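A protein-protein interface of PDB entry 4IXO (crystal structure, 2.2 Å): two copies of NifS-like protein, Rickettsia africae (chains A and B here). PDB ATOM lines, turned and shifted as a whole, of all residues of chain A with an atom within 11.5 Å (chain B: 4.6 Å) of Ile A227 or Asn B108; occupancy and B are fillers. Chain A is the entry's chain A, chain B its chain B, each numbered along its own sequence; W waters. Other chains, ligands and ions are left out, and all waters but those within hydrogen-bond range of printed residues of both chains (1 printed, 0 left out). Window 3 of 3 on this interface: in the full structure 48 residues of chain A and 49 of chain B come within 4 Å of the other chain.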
ATOM      1  N   THR A  75       8.606   8.746   1.773  1.00  0.00           N
ATOM      2  CA  THR A  75       8.948  10.151   1.999  1.00  0.00           C
ATOM      3  C   THR A  75       8.181  10.680   3.233  1.00  0.00           C
ATOM      4  O   THR A  75       6.953  10.668   3.251  1.00  0.00           O
ATOM      5  CB  THR A  75       8.595  11.003   0.775  1.00  0.00           C
ATOM      6  OG1 THR A  75       9.364  10.555  -0.344  1.00  0.00           O
ATOM      7  CG2 THR A  75       8.891  12.451   1.039  1.00  0.00           C
ATOM      8  N   PHE A  76       8.909  11.099   4.260  1.00  0.00           N
ATOM      9  CA  PHE A  76       8.277  11.629   5.471  1.00  0.00           C
ATOM     10  C   PHE A  76       7.779  13.058   5.249  1.00  0.00           C
ATOM     11  O   PHE A  76       8.546  13.935   4.795  1.00  0.00           O
ATOM     12  CB  PHE A  76       9.244  11.602   6.660  1.00  0.00           C
ATOM     13  CG  PHE A  76       9.610  10.211   7.108  1.00  0.00           C
ATOM     14  CD1 PHE A  76       8.628   9.313   7.485  1.00  0.00           C
ATOM     15  CD2 PHE A  76      10.942   9.789   7.119  1.00  0.00           C
ATOM     16  CE1 PHE A  76       8.964   8.020   7.878  1.00  0.00           C
ATOM     17  CE2 PHE A  76      11.282   8.537   7.536  1.00  0.00           C
ATOM     18  CZ  PHE A  76      10.292   7.640   7.909  1.00  0.00           C
ATOM     19  N   GLU A  82      -0.344  16.847   3.775  1.00  0.00           N
ATOM     20  CA  GLU A  82       0.818  17.202   2.964  1.00  0.00           C
ATOM     21  C   GLU A  82       1.121  16.110   1.956  1.00  0.00           C
ATOM     22  O   GLU A  82       1.438  16.401   0.809  1.00  0.00           O
ATOM     23  CB  GLU A  82       2.066  17.492   3.825  1.00  0.00           C
ATOM     24  CG  GLU A  82       3.233  18.031   3.028  1.00  0.00           C
ATOM     25  CD  GLU A  82       4.529  18.195   3.827  1.00  0.00           C
ATOM     26  OE1 GLU A  82       4.503  18.304   5.058  1.00  0.00           O
ATOM     27  OE2 GLU A  82       5.593  18.227   3.197  1.00  0.00           O
ATOM     28  N   LEU A  86       1.201  16.479  -2.125  1.00  0.00           N
ATOM     29  CA  LEU A  86       2.419  16.174  -2.846  1.00  0.00           C
ATOM     30  C   LEU A  86       2.151  15.247  -4.020  1.00  0.00           C
ATOM     31  O   LEU A  86       2.569  15.559  -5.140  1.00  0.00           O
ATOM     32  CB  LEU A  86       3.462  15.558  -1.903  1.00  0.00           C
ATOM     33  CG  LEU A  86       4.769  15.087  -2.536  1.00  0.00           C
ATOM     34  CD1 LEU A  86       5.537  16.256  -3.157  1.00  0.00           C
ATOM     35  CD2 LEU A  86       5.611  14.424  -1.477  1.00  0.00           C
ATOM     36  N   ASN A  90       1.934  16.355  -8.227  1.00  0.00           N
ATOM     37  CA  ASN A  90       2.766  15.659  -9.165  1.00  0.00           C
ATOM     38  C   ASN A  90       2.050  15.197 -10.434  1.00  0.00           C
ATOM     39  O   ASN A  90       2.699  14.810 -11.396  1.00  0.00           O
ATOM     40  CB  ASN A  90       3.475  14.507  -8.477  1.00  0.00           C
ATOM     41  CG  ASN A  90       4.847  14.899  -7.983  1.00  0.00           C
ATOM     42  OD1 ASN A  90       5.828  14.718  -8.681  1.00  0.00           O
ATOM     43  ND2 ASN A  90       4.920  15.455  -6.785  1.00  0.00           N
ATOM     44  N   GLN A 221       9.755   9.266 -10.134  1.00  0.00           N
ATOM     45  CA  GLN A 221      10.461  10.349  -9.439  1.00  0.00           C
ATOM     46  C   GLN A 221       9.454  11.397  -8.981  1.00  0.00           C
ATOM     47  O   GLN A 221       8.816  12.047  -9.788  1.00  0.00           O
ATOM     48  CB  GLN A 221      11.509  11.004 -10.354  1.00  0.00           C
ATOM     49  CG  GLN A 221      12.261  12.183  -9.696  1.00  0.00           C
ATOM     50  CD  GLN A 221      13.110  11.750  -8.489  1.00  0.00           C
ATOM     51  OE1 GLN A 221      13.948  10.844  -8.597  1.00  0.00           O
ATOM     52  NE2 GLN A 221      12.881  12.375  -7.325  1.00  0.00           N
ATOM     53  N   ILE A 222       9.291  11.537  -7.679  1.00  0.00           N
ATOM     54  CA  ILE A 222       8.408  12.574  -7.146  1.00  0.00           C
ATOM     55  C   ILE A 222       9.143  13.925  -7.211  1.00  0.00           C
ATOM     56  O   ILE A 222      10.269  14.014  -6.809  1.00  0.00           O
ATOM     57  CB  ILE A 222       8.036  12.286  -5.693  1.00  0.00           C
ATOM     58  CG1 ILE A 222       7.338  10.930  -5.518  1.00  0.00           C
ATOM     59  CG2 ILE A 222       7.168  13.417  -5.153  1.00  0.00           C
ATOM     60  CD1 ILE A 222       5.932  10.859  -6.060  1.00  0.00           C
ATOM     61  N   THR A 223       8.503  14.946  -7.757  1.00  0.00           N
ATOM     62  CA  THR A 223       9.025  16.287  -7.786  1.00  0.00           C
ATOM     63  C   THR A 223       8.607  16.943  -6.466  1.00  0.00           C
ATOM     64  O   THR A 223       7.467  16.805  -6.072  1.00  0.00           O
ATOM     65  CB  THR A 223       8.408  17.086  -8.960  1.00  0.00           C
ATOM     66  OG1 THR A 223       9.033  16.706 -10.184  1.00  0.00           O
ATOM     67  CG2 THR A 223       8.634  18.563  -8.812  1.00  0.00           C
ATOM     68  N   PRO A 224       9.525  17.676  -5.808  1.00  0.00           N
ATOM     69  CA  PRO A 224       9.203  18.270  -4.504  1.00  0.00           C
ATOM     70  C   PRO A 224       8.245  19.445  -4.596  1.00  0.00           C
ATOM     71  O   PRO A 224       8.274  20.203  -5.557  1.00  0.00           O
ATOM     72  CB  PRO A 224      10.555  18.756  -3.984  1.00  0.00           C
ATOM     73  CG  PRO A 224      11.348  19.050  -5.252  1.00  0.00           C
ATOM     74  CD  PRO A 224      10.893  18.001  -6.241  1.00  0.00           C
ATOM     75  N   MET A 225       7.416  19.593  -3.573  1.00  0.00           N
ATOM     76  CA  MET A 225       6.755  20.873  -3.322  1.00  0.00           C
ATOM     77  C   MET A 225       7.674  21.812  -2.506  1.00  0.00           C
ATOM     78  O   MET A 225       7.649  23.013  -2.679  1.00  0.00           O
ATOM     79  CB  MET A 225       5.491  20.663  -2.525  1.00  0.00           C
ATOM     80  CG  MET A 225       4.362  19.993  -3.281  1.00  0.00           C
ATOM     81  SD  MET A 225       3.130  19.512  -2.056  1.00  0.00           S
ATOM     82  CE  MET A 225       2.568  21.148  -1.513  1.00  0.00           C
ATOM     83  N   ILE A 226       8.448  21.244  -1.585  1.00  0.00           N
ATOM     84  CA  ILE A 226       9.227  22.031  -0.631  1.00  0.00           C
ATOM     85  C   ILE A 226      10.713  21.805  -0.838  1.00  0.00           C
ATOM     86  O   ILE A 226      11.216  20.693  -0.613  1.00  0.00           O
ATOM     87  CB  ILE A 226       8.830  21.659   0.799  1.00  0.00           C
ATOM     88  CG1 ILE A 226       7.335  21.922   1.010  1.00  0.00           C
ATOM     89  CG2 ILE A 226       9.652  22.447   1.814  1.00  0.00           C
ATOM     90  CD1 ILE A 226       6.826  21.475   2.361  1.00  0.00           C
ATOM     91  N   ILE A 227      11.415  22.866  -1.225  1.00  0.00           N
ATOM     92  CA  ILE A 227      12.826  22.780  -1.534  1.00  0.00           C
ATOM     93  C   ILE A 227      13.676  23.461  -0.501  1.00  0.00           C
ATOM     94  O   ILE A 227      13.191  24.252   0.320  1.00  0.00           O
ATOM     95  CB  ILE A 227      13.153  23.362  -2.920  1.00  0.00           C
ATOM     96  CG1 ILE A 227      12.810  24.841  -2.977  1.00  0.00           C
ATOM     97  CG2 ILE A 227      12.413  22.593  -3.999  1.00  0.00           C
ATOM     98  CD1 ILE A 227      13.358  25.539  -4.178  1.00  0.00           C
ATOM     99  N   GLY A 228      14.964  23.133  -0.528  1.00  0.00           N
ATOM    100  CA  GLY A 228      15.924  23.659   0.441  1.00  0.00           C
ATOM    101  C   GLY A 228      17.104  22.737   0.648  1.00  0.00           C
ATOM    102  O   GLY A 228      17.865  22.459  -0.279  1.00  0.00           O
ATOM    103  N   GLY A 229      17.233  22.240   1.860  1.00  0.00           N
ATOM    104  CA  GLY A 229      18.384  21.437   2.236  1.00  0.00           C
ATOM    105  C   GLY A 229      18.495  20.018   1.668  1.00  0.00           C
ATOM    106  O   GLY A 229      19.480  19.345   1.943  1.00  0.00           O
ATOM    107  N   GLY A 230      17.534  19.522   0.901  1.00  0.00           N
ATOM    108  CA  GLY A 230      17.731  18.190   0.288  1.00  0.00           C
ATOM    109  C   GLY A 230      17.369  16.961   1.140  1.00  0.00           C
ATOM    110  O   GLY A 230      17.690  15.830   0.778  1.00  0.00           O
ATOM    111  N   GLN A 231      16.666  17.170   2.240  1.00  0.00           N
ATOM    112  CA  GLN A 231      16.192  16.080   3.059  1.00  0.00           C
ATOM    113  C   GLN A 231      15.245  15.210   2.249  1.00  0.00           C
ATOM    114  O   GLN A 231      14.649  15.658   1.228  1.00  0.00           O
ATOM    115  CB  GLN A 231      15.477  16.590   4.319  1.00  0.00           C
ATOM    116  CG  GLN A 231      16.383  17.318   5.321  1.00  0.00           C
ATOM    117  CD  GLN A 231      16.539  18.802   5.035  1.00  0.00           C
ATOM    118  OE1 GLN A 231      16.115  19.319   3.987  1.00  0.00           O
ATOM    119  NE2 GLN A 231      17.152  19.509   5.982  1.00  0.00           N
ATOM    120  N   GLU A 232      15.127  13.973   2.702  1.00  0.00           N
ATOM    121  CA  GLU A 232      14.307  12.960   2.018  1.00  0.00           C
ATOM    122  C   GLU A 232      14.643  12.849   0.516  1.00  0.00           C
ATOM    123  O   GLU A 232      13.748  12.808  -0.330  1.00  0.00           O
ATOM    124  CB  GLU A 232      12.820  13.249   2.225  1.00  0.00           C
ATOM    125  CG  GLU A 232      12.374  13.202   3.685  1.00  0.00           C
ATOM    126  CD  GLU A 232      12.514  11.808   4.299  1.00  0.00           C
ATOM    127  OE1 GLU A 232      11.686  10.920   3.985  1.00  0.00           O
ATOM    128  OE2 GLU A 232      13.472  11.608   5.091  1.00  0.00           O
ATOM    129  N   LYS A 233      15.938  12.810   0.209  1.00  0.00           N
ATOM    130  CA  LYS A 233      16.448  12.702  -1.163  1.00  0.00           C
ATOM    131  C   LYS A 233      15.915  13.797  -2.082  1.00  0.00           C
ATOM    132  O   LYS A 233      15.621  13.558  -3.250  1.00  0.00           O
ATOM    133  CB  LYS A 233      16.129  11.316  -1.738  1.00  0.00           C
ATOM    134  CG  LYS A 233      16.723  10.178  -0.921  1.00  0.00           C
ATOM    135  CD  LYS A 233      16.232   8.849  -1.463  1.00  0.00           C
ATOM    136  CE  LYS A 233      17.014   7.672  -0.913  1.00  0.00           C
ATOM    137  NZ  LYS A 233      16.412   6.395  -1.435  1.00  0.00           N
ATOM    138  N   SER A 234      15.784  14.994  -1.514  1.00  0.00           N
ATOM    139  CA  SER A 234      15.333  16.206  -2.207  1.00  0.00           C
ATOM    140  C   SER A 234      13.873  16.171  -2.651  1.00  0.00           C
ATOM    141  O   SER A 234      13.478  16.971  -3.477  1.00  0.00           O
ATOM    142  CB  SER A 234      16.251  16.566  -3.381  1.00  0.00           C
ATOM    143  OG  SER A 234      17.573  16.796  -2.916  1.00  0.00           O
ATOM    144  N   VAL A 235      13.079  15.262  -2.091  1.00  0.00           N
ATOM    145  CA  VAL A 235      11.643  15.221  -2.367  1.00  0.00           C
ATOM    146  C   VAL A 235      10.875  16.099  -1.384  1.00  0.00           C
ATOM    147  O   VAL A 235       9.745  16.514  -1.656  1.00  0.00           O
ATOM    148  CB  VAL A 235      11.106  13.759  -2.327  1.00  0.00           C
ATOM    149  CG1 VAL A 235       9.600  13.711  -2.504  1.00  0.00           C
ATOM    150  CG2 VAL A 235      11.782  12.917  -3.409  1.00  0.00           C
ATOM    151  N   ARG A 236      11.478  16.392  -0.236  1.00  0.00           N
ATOM    152  CA  ARG A 236      10.779  17.071   0.826  1.00  0.00           C
ATOM    153  C   ARG A 236      11.796  17.635   1.798  1.00  0.00           C
ATOM    154  O   ARG A 236      12.253  16.954   2.722  1.00  0.00           O
ATOM    155  CB  ARG A 236       9.788  16.087   1.499  1.00  0.00           C
ATOM    156  CG  ARG A 236       8.645  16.728   2.270  1.00  0.00           C
ATOM    157  CD  ARG A 236       9.119  17.175   3.643  1.00  0.00           C
ATOM    158  NE  ARG A 236       8.089  17.887   4.372  1.00  0.00           N
ATOM    159  CZ  ARG A 236       8.284  18.447   5.559  1.00  0.00           C
ATOM    160  NH1 ARG A 236       9.465  18.355   6.156  1.00  0.00           N
ATOM    161  NH2 ARG A 236       7.298  19.104   6.155  1.00  0.00           N
ATOM    162  N   SER A 237      12.156  18.892   1.583  1.00  0.00           N
ATOM    163  CA  SER A 237      13.166  19.567   2.398  1.00  0.00           C
ATOM    164  C   SER A 237      12.571  20.092   3.709  1.00  0.00           C
ATOM    165  O   SER A 237      11.345  20.159   3.882  1.00  0.00           O
ATOM    166  CB  SER A 237      13.820  20.720   1.621  1.00  0.00           C
ATOM    167  OG  SER A 237      14.581  20.235   0.520  1.00  0.00           O
ATOM    168  N   GLY A 238      13.463  20.474   4.607  1.00  0.00           N
ATOM    169  CA  GLY A 238      13.111  20.922   5.947  1.00  0.00           C
ATOM    170  C   GLY A 238      13.708  19.948   6.928  1.00  0.00           C
ATOM    171  O   GLY A 238      13.827  18.741   6.626  1.00  0.00           O
ATOM    172  N   THR A 239      14.103  20.450   8.102  1.00  0.00           N
ATOM    173  CA  THR A 239      14.666  19.548   9.122  1.00  0.00           C
ATOM    174  C   THR A 239      13.590  18.520   9.497  1.00  0.00           C
ATOM    175  O   THR A 239      12.449  18.883   9.768  1.00  0.00           O
ATOM    176  CB  THR A 239      15.152  20.320  10.363  1.00  0.00           C
ATOM    177  OG1 THR A 239      16.122  21.298   9.959  1.00  0.00           O
ATOM    178  CG2 THR A 239      15.788  19.365  11.378  1.00  0.00           C
ATOM    179  N   THR B  81      11.708  26.025   6.743  1.00  0.00           N
ATOM    180  CA  THR B  81      11.816  25.725   5.355  1.00  0.00           C
ATOM    181  C   THR B  81      10.453  25.828   4.689  1.00  0.00           C
ATOM    182  O   THR B  81      10.331  26.436   3.607  1.00  0.00           O
ATOM    183  CB  THR B  81      12.375  24.294   5.143  1.00  0.00           C
ATOM    184  OG1 THR B  81      13.719  24.233   5.638  1.00  0.00           O
ATOM    185  CG2 THR B  81      12.365  23.915   3.689  1.00  0.00           C
ATOM    186  N   ASN B  85       9.374  28.514   1.777  1.00  0.00           N
ATOM    187  CA  ASN B  85       8.815  28.072   0.487  1.00  0.00           C
ATOM    188  C   ASN B  85       7.464  28.736   0.214  1.00  0.00           C
ATOM    189  O   ASN B  85       7.191  29.145  -0.903  1.00  0.00           O
ATOM    190  CB  ASN B  85       8.652  26.557   0.403  1.00  0.00           C
ATOM    191  CG  ASN B  85       9.913  25.867  -0.041  1.00  0.00           C
ATOM    192  OD1 ASN B  85      10.015  25.397  -1.169  1.00  0.00           O
ATOM    193  ND2 ASN B  85      10.887  25.811   0.842  1.00  0.00           N
ATOM    194  N   LEU B 104      19.406  27.810   2.238  1.00  0.00           N
ATOM    195  CA  LEU B 104      19.032  27.119   1.002  1.00  0.00           C
ATOM    196  C   LEU B 104      17.525  27.098   0.734  1.00  0.00           C
ATOM    197  O   LEU B 104      17.103  27.071  -0.433  1.00  0.00           O
ATOM    198  CB  LEU B 104      19.587  25.679   0.973  1.00  0.00           C
ATOM    199  CG  LEU B 104      21.103  25.563   0.807  1.00  0.00           C
ATOM    200  CD1 LEU B 104      21.522  24.113   0.939  1.00  0.00           C
ATOM    201  CD2 LEU B 104      21.568  26.140  -0.529  1.00  0.00           C
ATOM    202  N   SER B 105      16.713  27.127   1.798  1.00  0.00           N
ATOM    203  CA  SER B 105      15.259  27.166   1.667  1.00  0.00           C
ATOM    204  C   SER B 105      14.733  28.408   0.925  1.00  0.00           C
ATOM    205  O   SER B 105      13.590  28.410   0.481  1.00  0.00           O
ATOM    206  CB  SER B 105      14.556  27.001   3.019  1.00  0.00           C
ATOM    207  OG  SER B 105      14.890  27.995   3.969  1.00  0.00           O
ATOM    208  N   ILE B 106      15.542  29.468   0.830  1.00  0.00           N
ATOM    209  CA  ILE B 106      15.240  30.651   0.005  1.00  0.00           C
ATOM    210  C   ILE B 106      16.135  30.593  -1.236  1.00  0.00           C
ATOM    211  O   ILE B 106      15.667  30.819  -2.347  1.00  0.00           O
ATOM    212  CB  ILE B 106      15.563  31.963   0.733  1.00  0.00           C
ATOM    213  CG1 ILE B 106      14.704  32.153   1.990  1.00  0.00           C
ATOM    214  CG2 ILE B 106      15.431  33.179  -0.191  1.00  0.00           C
ATOM    215  CD1 ILE B 106      13.275  32.567   1.740  1.00  0.00           C
ATOM    216  N   TYR B 107      17.422  30.310  -1.029  1.00  0.00           N
ATOM    217  CA  TYR B 107      18.424  30.401  -2.077  1.00  0.00           C
ATOM    218  C   TYR B 107      18.125  29.485  -3.250  1.00  0.00           C
ATOM    219  O   TYR B 107      18.251  29.898  -4.428  1.00  0.00           O
ATOM    220  CB  TYR B 107      19.810  30.087  -1.526  1.00  0.00           C
ATOM    221  CG  TYR B 107      20.968  30.476  -2.440  1.00  0.00           C
ATOM    222  CD1 TYR B 107      21.338  31.789  -2.596  1.00  0.00           C
ATOM    223  CD2 TYR B 107      21.663  29.506  -3.162  1.00  0.00           C
ATOM    224  CE1 TYR B 107      22.392  32.139  -3.424  1.00  0.00           C
ATOM    225  CE2 TYR B 107      22.717  29.831  -3.998  1.00  0.00           C
ATOM    226  CZ  TYR B 107      23.082  31.157  -4.123  1.00  0.00           C
ATOM    227  OH  TYR B 107      24.137  31.498  -4.929  1.00  0.00           O
ATOM    228  N   ASN B 108      17.695  28.258  -2.960  1.00  0.00           N
ATOM    229  CA  ASN B 108      17.494  27.284  -4.045  1.00  0.00           C
ATOM    230  C   ASN B 108      16.306  27.572  -4.957  1.00  0.00           C
ATOM    231  O   ASN B 108      16.156  26.935  -6.013  1.00  0.00           O
ATOM    232  CB  ASN B 108      17.437  25.864  -3.503  1.00  0.00           C
ATOM    233  CG  ASN B 108      18.818  25.282  -3.274  1.00  0.00           C
ATOM    234  OD1 ASN B 108      19.810  25.805  -3.759  1.00  0.00           O
ATOM    235  ND2 ASN B 108      18.882  24.206  -2.538  1.00  0.00           N
ATOM    236  N   HIS B 109      15.480  28.536  -4.577  1.00  0.00           N
ATOM    237  CA  HIS B 109      14.467  29.036  -5.492  1.00  0.00           C
ATOM    238  C   HIS B 109      15.063  29.695  -6.748  1.00  0.00           C
ATOM    239  O   HIS B 109      14.343  29.962  -7.676  1.00  0.00           O
ATOM    240  CB  HIS B 109      13.493  29.978  -4.776  1.00  0.00           C
ATOM    241  CG  HIS B 109      12.661  29.280  -3.762  1.00  0.00           C
ATOM    242  ND1 HIS B 109      11.453  28.704  -4.069  1.00  0.00           N
ATOM    243  CD2 HIS B 109      12.911  28.975  -2.465  1.00  0.00           C
ATOM    244  CE1 HIS B 109      10.969  28.106  -2.994  1.00  0.00           C
ATOM    245  NE2 HIS B 109      11.837  28.253  -2.011  1.00  0.00           N
ATOM    246  N   ILE B 110      16.372  29.941  -6.786  1.00  0.00           N
ATOM    247  CA  ILE B 110      17.051  30.324  -8.018  1.00  0.00           C
ATOM    248  C   ILE B 110      16.776  29.343  -9.145  1.00  0.00           C
ATOM    249  O   ILE B 110      16.752  29.703 -10.303  1.00  0.00           O
ATOM    250  CB  ILE B 110      18.573  30.373  -7.783  1.00  0.00           C
ATOM    251  CG1 ILE B 110      18.925  31.601  -6.944  1.00  0.00           C
ATOM    252  CG2 ILE B 110      19.350  30.373  -9.097  1.00  0.00           C
ATOM    253  CD1 ILE B 110      20.280  31.516  -6.300  1.00  0.00           C
ATOM    254  N   ASN B 111      16.587  28.074  -8.778  1.00  0.00           N
ATOM    255  CA  ASN B 111      16.424  27.001  -9.747  1.00  0.00           C
ATOM    256  C   ASN B 111      14.987  26.793 -10.166  1.00  0.00           C
ATOM    257  O   ASN B 111      14.734  25.927 -10.989  1.00  0.00           O
ATOM    258  CB  ASN B 111      16.959  25.682  -9.175  1.00  0.00           C
ATOM    259  CG  ASN B 111      18.410  25.770  -8.798  1.00  0.00           C
ATOM    260  OD1 ASN B 111      19.212  26.295  -9.550  1.00  0.00           O
ATOM    261  ND2 ASN B 111      18.755  25.284  -7.604  1.00  0.00           N
ATOM    262  N   TYR B 112      14.052  27.563  -9.598  1.00  0.00           N
ATOM    263  CA  TYR B 112      12.643  27.402  -9.921  1.00  0.00           C
ATOM    264  C   TYR B 112      11.884  28.654 -10.295  1.00  0.00           C
ATOM    265  O   TYR B 112      11.041  28.616 -11.195  1.00  0.00           O
ATOM    266  CB  TYR B 112      11.917  26.744  -8.764  1.00  0.00           C
ATOM    267  CG  TYR B 112      12.337  25.319  -8.524  1.00  0.00           C
ATOM    268  CD1 TYR B 112      13.417  25.028  -7.704  1.00  0.00           C
ATOM    269  CD2 TYR B 112      11.630  24.256  -9.099  1.00  0.00           C
ATOM    270  CE1 TYR B 112      13.802  23.733  -7.471  1.00  0.00           C
ATOM    271  CE2 TYR B 112      12.010  22.937  -8.868  1.00  0.00           C
ATOM    272  CZ  TYR B 112      13.088  22.682  -8.042  1.00  0.00           C
ATOM    273  OH  TYR B 112      13.465  21.374  -7.778  1.00  0.00           O
HETATM  274  O   HOH W   1      15.869  23.077   4.269  1.00  0.00           O
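O of Ile A227 sits at hydrogen-bond distance from ND2 of Asn B85 (2.8 Å).
ND2 of Asn B108 sits at hydrogen-bond distance from O of Gly A228.
The backbone NH of Gly A230 lies within hydrogen-bond range of the side-chain hydroxyl of Ser A237.
N of Ser A237 sits at hydrogen-bond distance from O of Ile A226.
SD of Met A225 sits close to N of Leu A86, 3.6 Å away.
The side-chain amide oxygen (OE1) of Gln A231 sits at hydrogen-bond distance from the backbone NH (N) of Gly A238, 3.0 Å away.
O of Asn B108 is in hydrogen-bond range of ND2 of Asn B111.
O of Ser B105 lies within hydrogen-bond range of NE2 of His B109 (3.1 Å).
Met A225 touches Asn B85.
CG2 of Ile A226 touches CG2 of Thr B81, at 3.6 Å.
Ile A226 touches Asn B85.
CG2 of Thr B81 touches O of Ile A227, 3.5 Å away.
O of Ile A227 touches CA of Ser B105 (3.8 Å).
CD1 of Ile A227 touches O of Asn B108, at 3.6 Å.
O of Leu B104 touches CA of Gly A228 (3.7 Å).
Gly A228 touches Ser B105 (CA to CA, 3.8 Å).
Ser A237 touches Thr B81 (C to CG2, 3.8 Å).
Gly A238 touches Thr B81 (CA to OG1, 3.4 Å).
Of chain B, only Thr B81 (3.5 Å), Asn B85 (2.8 Å), Ser B105 (3.8 Å), Asn B108 (3.6 Å), His B109 (3.7 Å) and Tyr B112 (3.6 Å) come within 4 Å of Ile A227.
Of the printed residues of chain B, Ser A237 touches Thr B81 (3.8 Å).
Of the printed residues of chain B, Gly A238 touches Thr B81.
Asn B85 touches three residues of chain A.
Ser B105 touches just these residues of chain A: Ile A227 (3.8 Å) and Gly A228 (3.8 Å).
No residue of chain A comes within 4 Å of Tyr B107.
Asn B108 touches just these residues of chain A: Ile A227 and Gly A228.
No residue of chain A comes within 4 Å of Asn B111.
The nearest residue of chain A that does not touch Asn B108 is Gly A229 (5.1 Å).
Hydrophobic or aromatic side chains of chain B that line the printed part of chain A: Leu B104, His B109 and Tyr B112.
Of the 24 printed residues of chain A, 6 touch a printed residue of chain B.
Hydrophobic or aromatic side chains of chain A within 4 Å of the printed part of chain B: Ile A226 and Ile A227.
Among the printed residues, no Asp or Glu carboxylate lies within 4 Å of a Lys or Arg side-chain nitrogen of the other chain.
No position is printed for both chains.
Of the 14 pairs that touch across the chains among the printed residues, none has its exchanged pair printed and touching as well.
Water W1 bridges OG1 of Thr B81 and N of Gly A229.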
